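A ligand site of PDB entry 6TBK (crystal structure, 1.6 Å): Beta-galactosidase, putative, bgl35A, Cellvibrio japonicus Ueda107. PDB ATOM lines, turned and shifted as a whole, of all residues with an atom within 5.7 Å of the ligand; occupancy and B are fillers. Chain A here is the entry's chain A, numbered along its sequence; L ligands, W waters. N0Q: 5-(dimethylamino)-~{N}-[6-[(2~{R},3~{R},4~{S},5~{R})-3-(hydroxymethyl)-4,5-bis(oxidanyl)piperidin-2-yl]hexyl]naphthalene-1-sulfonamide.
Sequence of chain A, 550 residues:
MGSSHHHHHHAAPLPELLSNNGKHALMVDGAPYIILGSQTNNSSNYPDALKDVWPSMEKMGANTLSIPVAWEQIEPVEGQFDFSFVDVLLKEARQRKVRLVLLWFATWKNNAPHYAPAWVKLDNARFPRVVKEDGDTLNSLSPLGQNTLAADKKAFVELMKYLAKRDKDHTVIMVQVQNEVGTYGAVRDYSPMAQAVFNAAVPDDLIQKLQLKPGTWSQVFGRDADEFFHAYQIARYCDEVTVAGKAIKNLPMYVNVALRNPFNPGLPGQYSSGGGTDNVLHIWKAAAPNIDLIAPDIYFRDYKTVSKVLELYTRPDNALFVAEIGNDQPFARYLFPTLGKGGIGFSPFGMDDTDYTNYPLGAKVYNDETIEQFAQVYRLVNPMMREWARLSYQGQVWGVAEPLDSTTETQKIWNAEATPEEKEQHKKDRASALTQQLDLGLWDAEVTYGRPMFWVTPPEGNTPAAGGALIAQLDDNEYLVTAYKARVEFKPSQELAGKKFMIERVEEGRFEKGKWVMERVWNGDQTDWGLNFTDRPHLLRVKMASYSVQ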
ATOM      1  N   GLN A  39     -16.568 -12.287   8.712  1.00  0.00           N
ATOM      2  CA  GLN A  39     -16.416 -13.745   8.940  1.00  0.00           C
ATOM      3  C   GLN A  39     -17.731 -14.258   9.504  1.00  0.00           C
ATOM      4  O   GLN A  39     -18.319 -13.662  10.383  1.00  0.00           O
ATOM      5  CB  GLN A  39     -15.191 -14.089   9.821  1.00  0.00           C
ATOM      6  CG  GLN A  39     -15.073 -15.583  10.028  1.00  0.00           C
ATOM      7  CD  GLN A  39     -13.869 -16.112  10.752  1.00  0.00           C
ATOM      8  OE1 GLN A  39     -13.933 -17.183  11.326  1.00  0.00           O
ATOM      9  NE2 GLN A  39     -12.778 -15.399  10.693  1.00  0.00           N
ATOM     10  N   ASN A  41     -20.075 -16.945  11.732  1.00  0.00           N
ATOM     11  CA  ASN A  41     -19.951 -17.810  12.917  1.00  0.00           C
ATOM     12  C   ASN A  41     -19.448 -19.203  12.517  1.00  0.00           C
ATOM     13  O   ASN A  41     -19.484 -19.574  11.306  1.00  0.00           O
ATOM     14  CB  ASN A  41     -21.306 -17.836  13.648  1.00  0.00           C
ATOM     15  CG  ASN A  41     -21.493 -16.627  14.520  1.00  0.00           C
ATOM     16  OD1 ASN A  41     -20.704 -16.351  15.426  1.00  0.00           O
ATOM     17  ND2 ASN A  41     -22.498 -15.860  14.217  1.00  0.00           N
ATOM     18  N   ASN A  42     -18.992 -19.988  13.483  1.00  0.00           N
ATOM     19  CA  ASN A  42     -18.227 -21.222  13.239  1.00  0.00           C
ATOM     20  C   ASN A  42     -19.076 -22.344  12.608  1.00  0.00           C
ATOM     21  O   ASN A  42     -18.486 -23.357  12.140  1.00  0.00           O
ATOM     22  CB  ASN A  42     -17.662 -21.758  14.555  1.00  0.00           C
ATOM     23  CG  ASN A  42     -16.440 -21.031  15.095  1.00  0.00           C
ATOM     24  OD1 ASN A  42     -16.105 -21.222  16.257  1.00  0.00           O
ATOM     25  ND2 ASN A  42     -15.822 -20.187  14.271  1.00  0.00           N
ATOM     26  N   PHE A 105     -10.234 -25.516   8.629  1.00  0.00           N
ATOM     27  CA  PHE A 105     -10.448 -25.974  10.021  1.00  0.00           C
ATOM     28  C   PHE A 105     -10.035 -27.436  10.048  1.00  0.00           C
ATOM     29  O   PHE A 105     -10.711 -28.240   9.381  1.00  0.00           O
ATOM     30  CB  PHE A 105     -11.905 -25.726  10.441  1.00  0.00           C
ATOM     31  CG  PHE A 105     -12.283 -24.348  10.890  1.00  0.00           C
ATOM     32  CD1 PHE A 105     -11.580 -23.219  10.535  1.00  0.00           C
ATOM     33  CD2 PHE A 105     -13.465 -24.159  11.605  1.00  0.00           C
ATOM     34  CE1 PHE A 105     -11.973 -21.957  10.958  1.00  0.00           C
ATOM     35  CE2 PHE A 105     -13.883 -22.913  11.986  1.00  0.00           C
ATOM     36  CZ  PHE A 105     -13.116 -21.799  11.668  1.00  0.00           C
ATOM     37  N   LYS A 109      -8.318 -26.140  15.456  1.00  0.00           N
ATOM     38  CA  LYS A 109      -9.347 -25.094  15.496  1.00  0.00           C
ATOM     39  C   LYS A 109      -9.492 -24.756  16.968  1.00  0.00           C
ATOM     40  O   LYS A 109      -9.921 -25.602  17.736  1.00  0.00           O
ATOM     41  CB  LYS A 109     -10.639 -25.577  14.831  1.00  0.00           C
ATOM     42  CG  LYS A 109     -11.577 -24.432  14.489  1.00  0.00           C
ATOM     43  CD  LYS A 109     -12.211 -23.790  15.756  1.00  0.00           C
ATOM     44  CE  LYS A 109     -13.227 -22.758  15.400  1.00  0.00           C
ATOM     45  NZ  LYS A 109     -13.519 -21.953  16.596  1.00  0.00           N
ATOM     46  N   ASN A 110      -8.942 -23.598  17.341  1.00  0.00           N
ATOM     47  CA  ASN A 110      -8.885 -23.133  18.736  1.00  0.00           C
ATOM     48  C   ASN A 110      -8.171 -24.206  19.587  1.00  0.00           C
ATOM     49  O   ASN A 110      -8.701 -24.575  20.634  1.00  0.00           O
ATOM     50  CB  ASN A 110     -10.264 -22.738  19.294  1.00  0.00           C
ATOM     51  CG  ASN A 110     -10.917 -21.553  18.597  1.00  0.00           C
ATOM     52  OD1 ASN A 110     -10.671 -21.228  17.410  1.00  0.00           O
ATOM     53  ND2 ASN A 110     -11.841 -20.944  19.327  1.00  0.00           N
ATOM     54  N   ASN A 179      -6.848 -22.969  12.311  1.00  0.00           N
ATOM     55  CA  ASN A 179      -7.512 -21.835  12.990  1.00  0.00           C
ATOM     56  C   ASN A 179      -7.036 -21.788  14.439  1.00  0.00           C
ATOM     57  O   ASN A 179      -7.420 -22.641  15.204  1.00  0.00           O
ATOM     58  CB  ASN A 179      -9.058 -21.911  12.910  1.00  0.00           C
ATOM     59  CG  ASN A 179      -9.763 -20.716  13.530  1.00  0.00           C
ATOM     60  OD1 ASN A 179      -9.877 -19.681  12.908  1.00  0.00           O
ATOM     61  ND2 ASN A 179     -10.247 -20.854  14.767  1.00  0.00           N
ATOM     62  N   GLU A 180      -6.293 -20.738  14.809  1.00  0.00           N
ATOM     63  CA  GLU A 180      -5.824 -20.532  16.202  1.00  0.00           C
ATOM     64  C   GLU A 180      -5.148 -21.819  16.711  1.00  0.00           C
ATOM     65  O   GLU A 180      -5.591 -22.477  17.660  1.00  0.00           O
ATOM     66  CB  GLU A 180      -6.925 -19.982  17.111  1.00  0.00           C
ATOM     67  CG  GLU A 180      -7.474 -18.634  16.648  1.00  0.00           C
ATOM     68  CD  GLU A 180      -8.194 -17.811  17.716  1.00  0.00           C
ATOM     69  OE1 GLU A 180      -8.537 -18.408  18.754  1.00  0.00           O
ATOM     70  OE2 GLU A 180      -8.409 -16.563  17.506  1.00  0.00           O
ATOM     71  N   TYR A 184      -3.939 -25.238  24.911  1.00  0.00           N
ATOM     72  CA  TYR A 184      -4.393 -24.742  26.224  1.00  0.00           C
ATOM     73  C   TYR A 184      -4.104 -25.846  27.212  1.00  0.00           C
ATOM     74  O   TYR A 184      -4.251 -27.063  26.780  1.00  0.00           O
ATOM     75  CB  TYR A 184      -5.873 -24.358  26.203  1.00  0.00           C
ATOM     76  CG  TYR A 184      -6.249 -23.175  25.343  1.00  0.00           C
ATOM     77  CD1 TYR A 184      -5.886 -21.904  25.738  1.00  0.00           C
ATOM     78  CD2 TYR A 184      -7.053 -23.294  24.209  1.00  0.00           C
ATOM     79  CE1 TYR A 184      -6.224 -20.785  24.983  1.00  0.00           C
ATOM     80  CE2 TYR A 184      -7.427 -22.190  23.438  1.00  0.00           C
ATOM     81  CZ  TYR A 184      -6.998 -20.919  23.831  1.00  0.00           C
ATOM     82  OH  TYR A 184      -7.231 -19.767  23.184  1.00  0.00           O
ATOM     83  N   ASN A 256      -3.833 -17.426  11.813  1.00  0.00           N
ATOM     84  CA  ASN A 256      -4.486 -16.446  12.688  1.00  0.00           C
ATOM     85  C   ASN A 256      -4.148 -16.810  14.121  1.00  0.00           C
ATOM     86  O   ASN A 256      -4.288 -17.934  14.540  1.00  0.00           O
ATOM     87  CB  ASN A 256      -6.010 -16.387  12.427  1.00  0.00           C
ATOM     88  CG  ASN A 256      -6.711 -17.694  12.680  1.00  0.00           C
ATOM     89  OD1 ASN A 256      -6.181 -18.766  12.350  1.00  0.00           O
ATOM     90  ND2 ASN A 256      -7.917 -17.566  13.224  1.00  0.00           N
ATOM     91  N   ALA A 258      -4.487 -16.755  18.203  1.00  0.00           N
ATOM     92  CA  ALA A 258      -5.179 -16.557  19.491  1.00  0.00           C
ATOM     93  C   ALA A 258      -4.233 -15.741  20.378  1.00  0.00           C
ATOM     94  O   ALA A 258      -3.225 -16.327  20.847  1.00  0.00           O
ATOM     95  CB  ALA A 258      -5.494 -17.854  20.156  1.00  0.00           C
ATOM     96  N   LEU A 259      -4.476 -14.455  20.487  1.00  0.00           N
ATOM     97  CA  LEU A 259      -3.468 -13.495  21.056  1.00  0.00           C
ATOM     98  C   LEU A 259      -3.307 -13.726  22.545  1.00  0.00           C
ATOM     99  O   LEU A 259      -4.291 -13.993  23.271  1.00  0.00           O
ATOM    100  CB  LEU A 259      -3.934 -12.064  20.837  1.00  0.00           C
ATOM    101  CG  LEU A 259      -4.095 -11.645  19.380  1.00  0.00           C
ATOM    102  CD1 LEU A 259      -4.647 -10.225  19.316  1.00  0.00           C
ATOM    103  CD2 LEU A 259      -2.743 -11.786  18.623  1.00  0.00           C
ATOM    104  N   ARG A 260      -2.082 -13.505  23.004  1.00  0.00           N
ATOM    105  CA  ARG A 260      -1.821 -13.297  24.436  1.00  0.00           C
ATOM    106  C   ARG A 260      -1.855 -11.785  24.646  1.00  0.00           C
ATOM    107  O   ARG A 260      -1.611 -11.067  23.684  1.00  0.00           O
ATOM    108  CB  ARG A 260      -0.473 -13.910  24.848  1.00  0.00           C
ATOM    109  CG  ARG A 260       0.729 -13.079  24.416  1.00  0.00           C
ATOM    110  CD  ARG A 260       1.971 -13.852  24.902  1.00  0.00           C
ATOM    111  NE  ARG A 260       3.102 -12.968  24.777  1.00  0.00           N
ATOM    112  CZ  ARG A 260       4.195 -13.039  25.513  1.00  0.00           C
ATOM    113  NH1 ARG A 260       4.357 -14.061  26.357  1.00  0.00           N
ATOM    114  NH2 ARG A 260       5.141 -12.117  25.343  1.00  0.00           N
ATOM    115  N   ASP A 297      -6.005 -11.902  15.978  1.00  0.00           N
ATOM    116  CA  ASP A 297      -7.479 -12.070  16.142  1.00  0.00           C
ATOM    117  C   ASP A 297      -7.767 -11.243  17.386  1.00  0.00           C
ATOM    118  O   ASP A 297      -7.424 -11.704  18.460  1.00  0.00           O
ATOM    119  CB  ASP A 297      -7.820 -13.533  16.414  1.00  0.00           C
ATOM    120  CG  ASP A 297      -7.672 -14.459  15.227  1.00  0.00           C
ATOM    121  OD1 ASP A 297      -7.485 -13.984  14.094  1.00  0.00           O
ATOM    122  OD2 ASP A 297      -7.741 -15.682  15.441  1.00  0.00           O
ATOM    123  N   TYR A 299      -9.786  -9.342  20.276  1.00  0.00           N
ATOM    124  CA  TYR A 299     -11.007  -9.241  21.108  1.00  0.00           C
ATOM    125  C   TYR A 299     -10.771  -8.370  22.351  1.00  0.00           C
ATOM    126  O   TYR A 299     -11.660  -8.146  23.195  1.00  0.00           O
ATOM    127  CB  TYR A 299     -11.474 -10.657  21.454  1.00  0.00           C
ATOM    128  CG  TYR A 299     -11.903 -11.438  20.231  1.00  0.00           C
ATOM    129  CD1 TYR A 299     -13.141 -11.194  19.649  1.00  0.00           C
ATOM    130  CD2 TYR A 299     -11.070 -12.308  19.579  1.00  0.00           C
ATOM    131  CE1 TYR A 299     -13.515 -11.841  18.476  1.00  0.00           C
ATOM    132  CE2 TYR A 299     -11.465 -13.011  18.430  1.00  0.00           C
ATOM    133  CZ  TYR A 299     -12.700 -12.764  17.857  1.00  0.00           C
ATOM    134  OH  TYR A 299     -13.106 -13.430  16.756  1.00  0.00           O
ATOM    135  N   PHE A 300      -9.577  -7.724  22.441  1.00  0.00           N
ATOM    136  CA  PHE A 300      -9.334  -6.659  23.447  1.00  0.00           C
ATOM    137  C   PHE A 300     -10.127  -5.408  23.012  1.00  0.00           C
ATOM    138  O   PHE A 300     -10.086  -5.035  21.817  1.00  0.00           O
ATOM    139  CB  PHE A 300      -7.834  -6.347  23.561  1.00  0.00           C
ATOM    140  CG  PHE A 300      -6.927  -7.547  23.720  1.00  0.00           C
ATOM    141  CD1 PHE A 300      -7.011  -8.381  24.804  1.00  0.00           C
ATOM    142  CD2 PHE A 300      -5.953  -7.835  22.778  1.00  0.00           C
ATOM    143  CE1 PHE A 300      -6.205  -9.503  24.931  1.00  0.00           C
ATOM    144  CE2 PHE A 300      -5.153  -8.962  22.887  1.00  0.00           C
ATOM    145  CZ  PHE A 300      -5.261  -9.794  23.968  1.00  0.00           C
ATOM    146  N   GLU A 324      -9.515 -11.472  12.375  1.00  0.00           N
ATOM    147  CA  GLU A 324     -10.773 -11.446  13.154  1.00  0.00           C
ATOM    148  C   GLU A 324     -10.723 -10.246  14.078  1.00  0.00           C
ATOM    149  O   GLU A 324      -9.602  -9.929  14.611  1.00  0.00           O
ATOM    150  CB  GLU A 324     -10.983 -12.666  14.056  1.00  0.00           C
ATOM    151  CG  GLU A 324     -10.982 -13.989  13.360  1.00  0.00           C
ATOM    152  CD  GLU A 324     -10.950 -15.170  14.330  1.00  0.00           C
ATOM    153  OE1 GLU A 324     -11.325 -14.914  15.533  1.00  0.00           O
ATOM    154  OE2 GLU A 324     -10.481 -16.302  13.952  1.00  0.00           O
ATOM    155  N   PHE A 349     -15.805 -10.660  13.213  1.00  0.00           N
ATOM    156  CA  PHE A 349     -16.241 -12.033  13.447  1.00  0.00           C
ATOM    157  C   PHE A 349     -17.702 -12.069  13.898  1.00  0.00           C
ATOM    158  O   PHE A 349     -18.116 -11.331  14.772  1.00  0.00           O
ATOM    159  CB  PHE A 349     -15.355 -12.644  14.528  1.00  0.00           C
ATOM    160  CG  PHE A 349     -15.677 -14.081  14.731  1.00  0.00           C
ATOM    161  CD1 PHE A 349     -15.115 -15.075  13.947  1.00  0.00           C
ATOM    162  CD2 PHE A 349     -16.652 -14.414  15.671  1.00  0.00           C
ATOM    163  CE1 PHE A 349     -15.499 -16.404  14.095  1.00  0.00           C
ATOM    164  CE2 PHE A 349     -17.021 -15.747  15.826  1.00  0.00           C
ATOM    165  CZ  PHE A 349     -16.447 -16.736  15.048  1.00  0.00           C
ATOM    166  N   TYR A 356     -26.503 -16.771  16.999  1.00  0.00           N
ATOM    167  CA  TYR A 356     -25.392 -16.990  17.949  1.00  0.00           C
ATOM    168  C   TYR A 356     -24.725 -15.636  18.190  1.00  0.00           C
ATOM    169  O   TYR A 356     -24.625 -14.924  17.225  1.00  0.00           O
ATOM    170  CB  TYR A 356     -24.339 -17.958  17.414  1.00  0.00           C
ATOM    171  CG  TYR A 356     -23.268 -18.234  18.418  1.00  0.00           C
ATOM    172  CD1 TYR A 356     -23.501 -19.174  19.432  1.00  0.00           C
ATOM    173  CD2 TYR A 356     -22.059 -17.553  18.382  1.00  0.00           C
ATOM    174  CE1 TYR A 356     -22.591 -19.420  20.418  1.00  0.00           C
ATOM    175  CE2 TYR A 356     -21.119 -17.869  19.345  1.00  0.00           C
ATOM    176  CZ  TYR A 356     -21.349 -18.763  20.366  1.00  0.00           C
ATOM    177  OH  TYR A 356     -20.424 -19.002  21.366  1.00  0.00           O
ATOM    178  N   ASN A 358     -21.135 -14.172  20.306  1.00  0.00           N
ATOM    179  CA  ASN A 358     -19.957 -14.575  21.122  1.00  0.00           C
ATOM    180  C   ASN A 358     -19.703 -13.581  22.245  1.00  0.00           C
ATOM    181  O   ASN A 358     -18.677 -13.701  22.899  1.00  0.00           O
ATOM    182  CB  ASN A 358     -18.715 -14.833  20.274  1.00  0.00           C
ATOM    183  CG  ASN A 358     -18.132 -13.583  19.684  1.00  0.00           C
ATOM    184  OD1 ASN A 358     -18.745 -12.534  19.807  1.00  0.00           O
ATOM    185  ND2 ASN A 358     -17.060 -13.750  18.935  1.00  0.00           N
ATOM    186  N   LEU A 361     -17.247 -11.485  24.198  1.00  0.00           N
ATOM    187  CA  LEU A 361     -16.207 -11.068  23.198  1.00  0.00           C
ATOM    188  C   LEU A 361     -16.823 -10.048  22.230  1.00  0.00           C
ATOM    189  O   LEU A 361     -16.248  -8.983  21.983  1.00  0.00           O
ATOM    190  CB  LEU A 361     -15.710 -12.286  22.417  1.00  0.00           C
ATOM    191  CG  LEU A 361     -14.956 -13.357  23.208  1.00  0.00           C
ATOM    192  CD1 LEU A 361     -14.204 -14.270  22.290  1.00  0.00           C
ATOM    193  CD2 LEU A 361     -13.994 -12.730  24.202  1.00  0.00           C
HETATM  194  C6  N0Q L   1      -9.837 -12.315  24.579  1.00  0.00           C
HETATM  195  N2  N0Q L   1      -8.886 -14.714  24.529  1.00  0.00           N
HETATM  196  CAP N0Q L   1     -10.859 -15.442  23.462  1.00  0.00           C
HETATM  197  CAO N0Q L   1     -11.175 -16.928  23.389  1.00  0.00           C
HETATM  198  CAN N0Q L   1     -10.741 -17.527  22.071  1.00  0.00           C
HETATM  199  CAM N0Q L   1     -11.383 -16.731  20.913  1.00  0.00           C
HETATM  200  CAL N0Q L   1     -11.883 -17.519  19.728  1.00  0.00           C
HETATM  201  CAA N0Q L   1     -12.226 -16.553  18.612  1.00  0.00           C
HETATM  202  NAB N0Q L   1     -11.358 -16.740  17.479  1.00  0.00           N
HETATM  203  CAI N0Q L   1     -11.482 -18.025  16.750  1.00  0.00           C
HETATM  204  CAJ N0Q L   1     -12.868 -18.007  16.134  1.00  0.00           C
HETATM  205  OAF N0Q L   1     -13.015 -19.172  15.343  1.00  0.00           O
HETATM  206  CAC N0Q L   1     -13.835 -17.959  17.266  1.00  0.00           C
HETATM  207  OAE N0Q L   1     -13.765 -19.191  18.007  1.00  0.00           O
HETATM  208  CAD N0Q L   1     -13.678 -16.738  18.113  1.00  0.00           C
HETATM  209  CAH N0Q L   1     -14.682 -16.621  19.227  1.00  0.00           C
HETATM  210  OAK N0Q L   1     -16.049 -16.405  18.666  1.00  0.00           O
HETATM  211  C1  N0Q L   1     -10.268 -15.075  24.818  1.00  0.00           C
HETATM  212  S3  N0Q L   1      -8.458 -13.163  24.641  1.00  0.00           S
HETATM  213  O4  N0Q L   1      -7.550 -12.737  23.520  1.00  0.00           O
HETATM  214  O5  N0Q L   1      -7.775 -13.019  25.899  1.00  0.00           O
HETATM  215  O   HOH W   1      -7.811 -10.764  21.623  1.00  0.00           O
HETATM  216  O   HOH W   2     -12.400 -18.663  12.858  1.00  0.00           O
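OE1 of Glu 324 is in salt-bridge range of NAB of the ligand.
The side-chain amide nitrogen (ND2) of Asn 358 is in hydrogen-bond range of an oxygen (OAK) of the ligand, 2.9 Å away.
OAE of the ligand lies within hydrogen-bond range of ND2 of Asn 110.
A nitrogen (NAB) of the ligand lies within salt-bridge range of the side-chain carboxylate of Glu 180 (3.0 Å).
NZ of Lys 109 sits at hydrogen-bond distance from OAF of the ligand.
ND2 of Asn 42 sits at hydrogen-bond distance from OAF of the ligand, at 3.2 Å.
An oxygen (OAF) of the ligand lies within hydrogen-bond range of the side-chain amide nitrogen (ND2) of Asn 179 (3.3 Å).
Leu 259 touches the ligand (O to O4, 3.5 Å).
Tyr 299 touches the ligand (OH to CAD, 3.6 Å).
Phe 300 touches the ligand (CZ to O4, 3.8 Å).
Phe 349 touches the ligand (CE2 to OAK, 3.1 Å).
Leu 361 touches the ligand.
Hydrophobic or aromatic side chains that line the ligand: Tyr 299, Phe 300, Phe 349 and Leu 361.
Within 4 Å of the ligand: Asn 42, Lys 109, Asn 110, Asn 179, Glu 180, Leu 259, Tyr 299, Phe 300, Glu 324, Phe 349, Asn 358 and Leu 361.
Along chain A the residues within 4 Å of the ligand span positions 42 to 361.
The nearest printed residue that does not touch the ligand is Asp 297 (4.3 Å).
Water W1 lies within hydrogen-bond range of O4 of the ligand, N of Tyr 299 and O of Asp 297.
The side-chain hydroxyl (OH) of Tyr 299 lies within hydrogen-bond range of the side-chain carboxylate (OE1) of Glu 324 (2.6 Å).
OE2 of Glu 324 lies within hydrogen-bond range of ND2 of Asn 256.
The side-chain amide oxygen of Asn 110 is in hydrogen-bond range of the side-chain amino group of Lys 109, 3.0 Å away.
The side-chain amide oxygen (OD1) of Asn 110 sits at hydrogen-bond distance from the side-chain amide nitrogen (ND2) of Asn 179 (2.7 Å).
The side-chain amide oxygen (OD1) of Asn 256 is in hydrogen-bond range of the backbone NH (N) of Glu 180.
The side-chain amide oxygen (OD1) of Asn 42 lies within hydrogen-bond range of the side-chain amino group (NZ) of Lys 109 (2.7 Å).
OD1 of Asn 179 is in hydrogen-bond range of ND2 of Asn 256 (2.9 Å).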
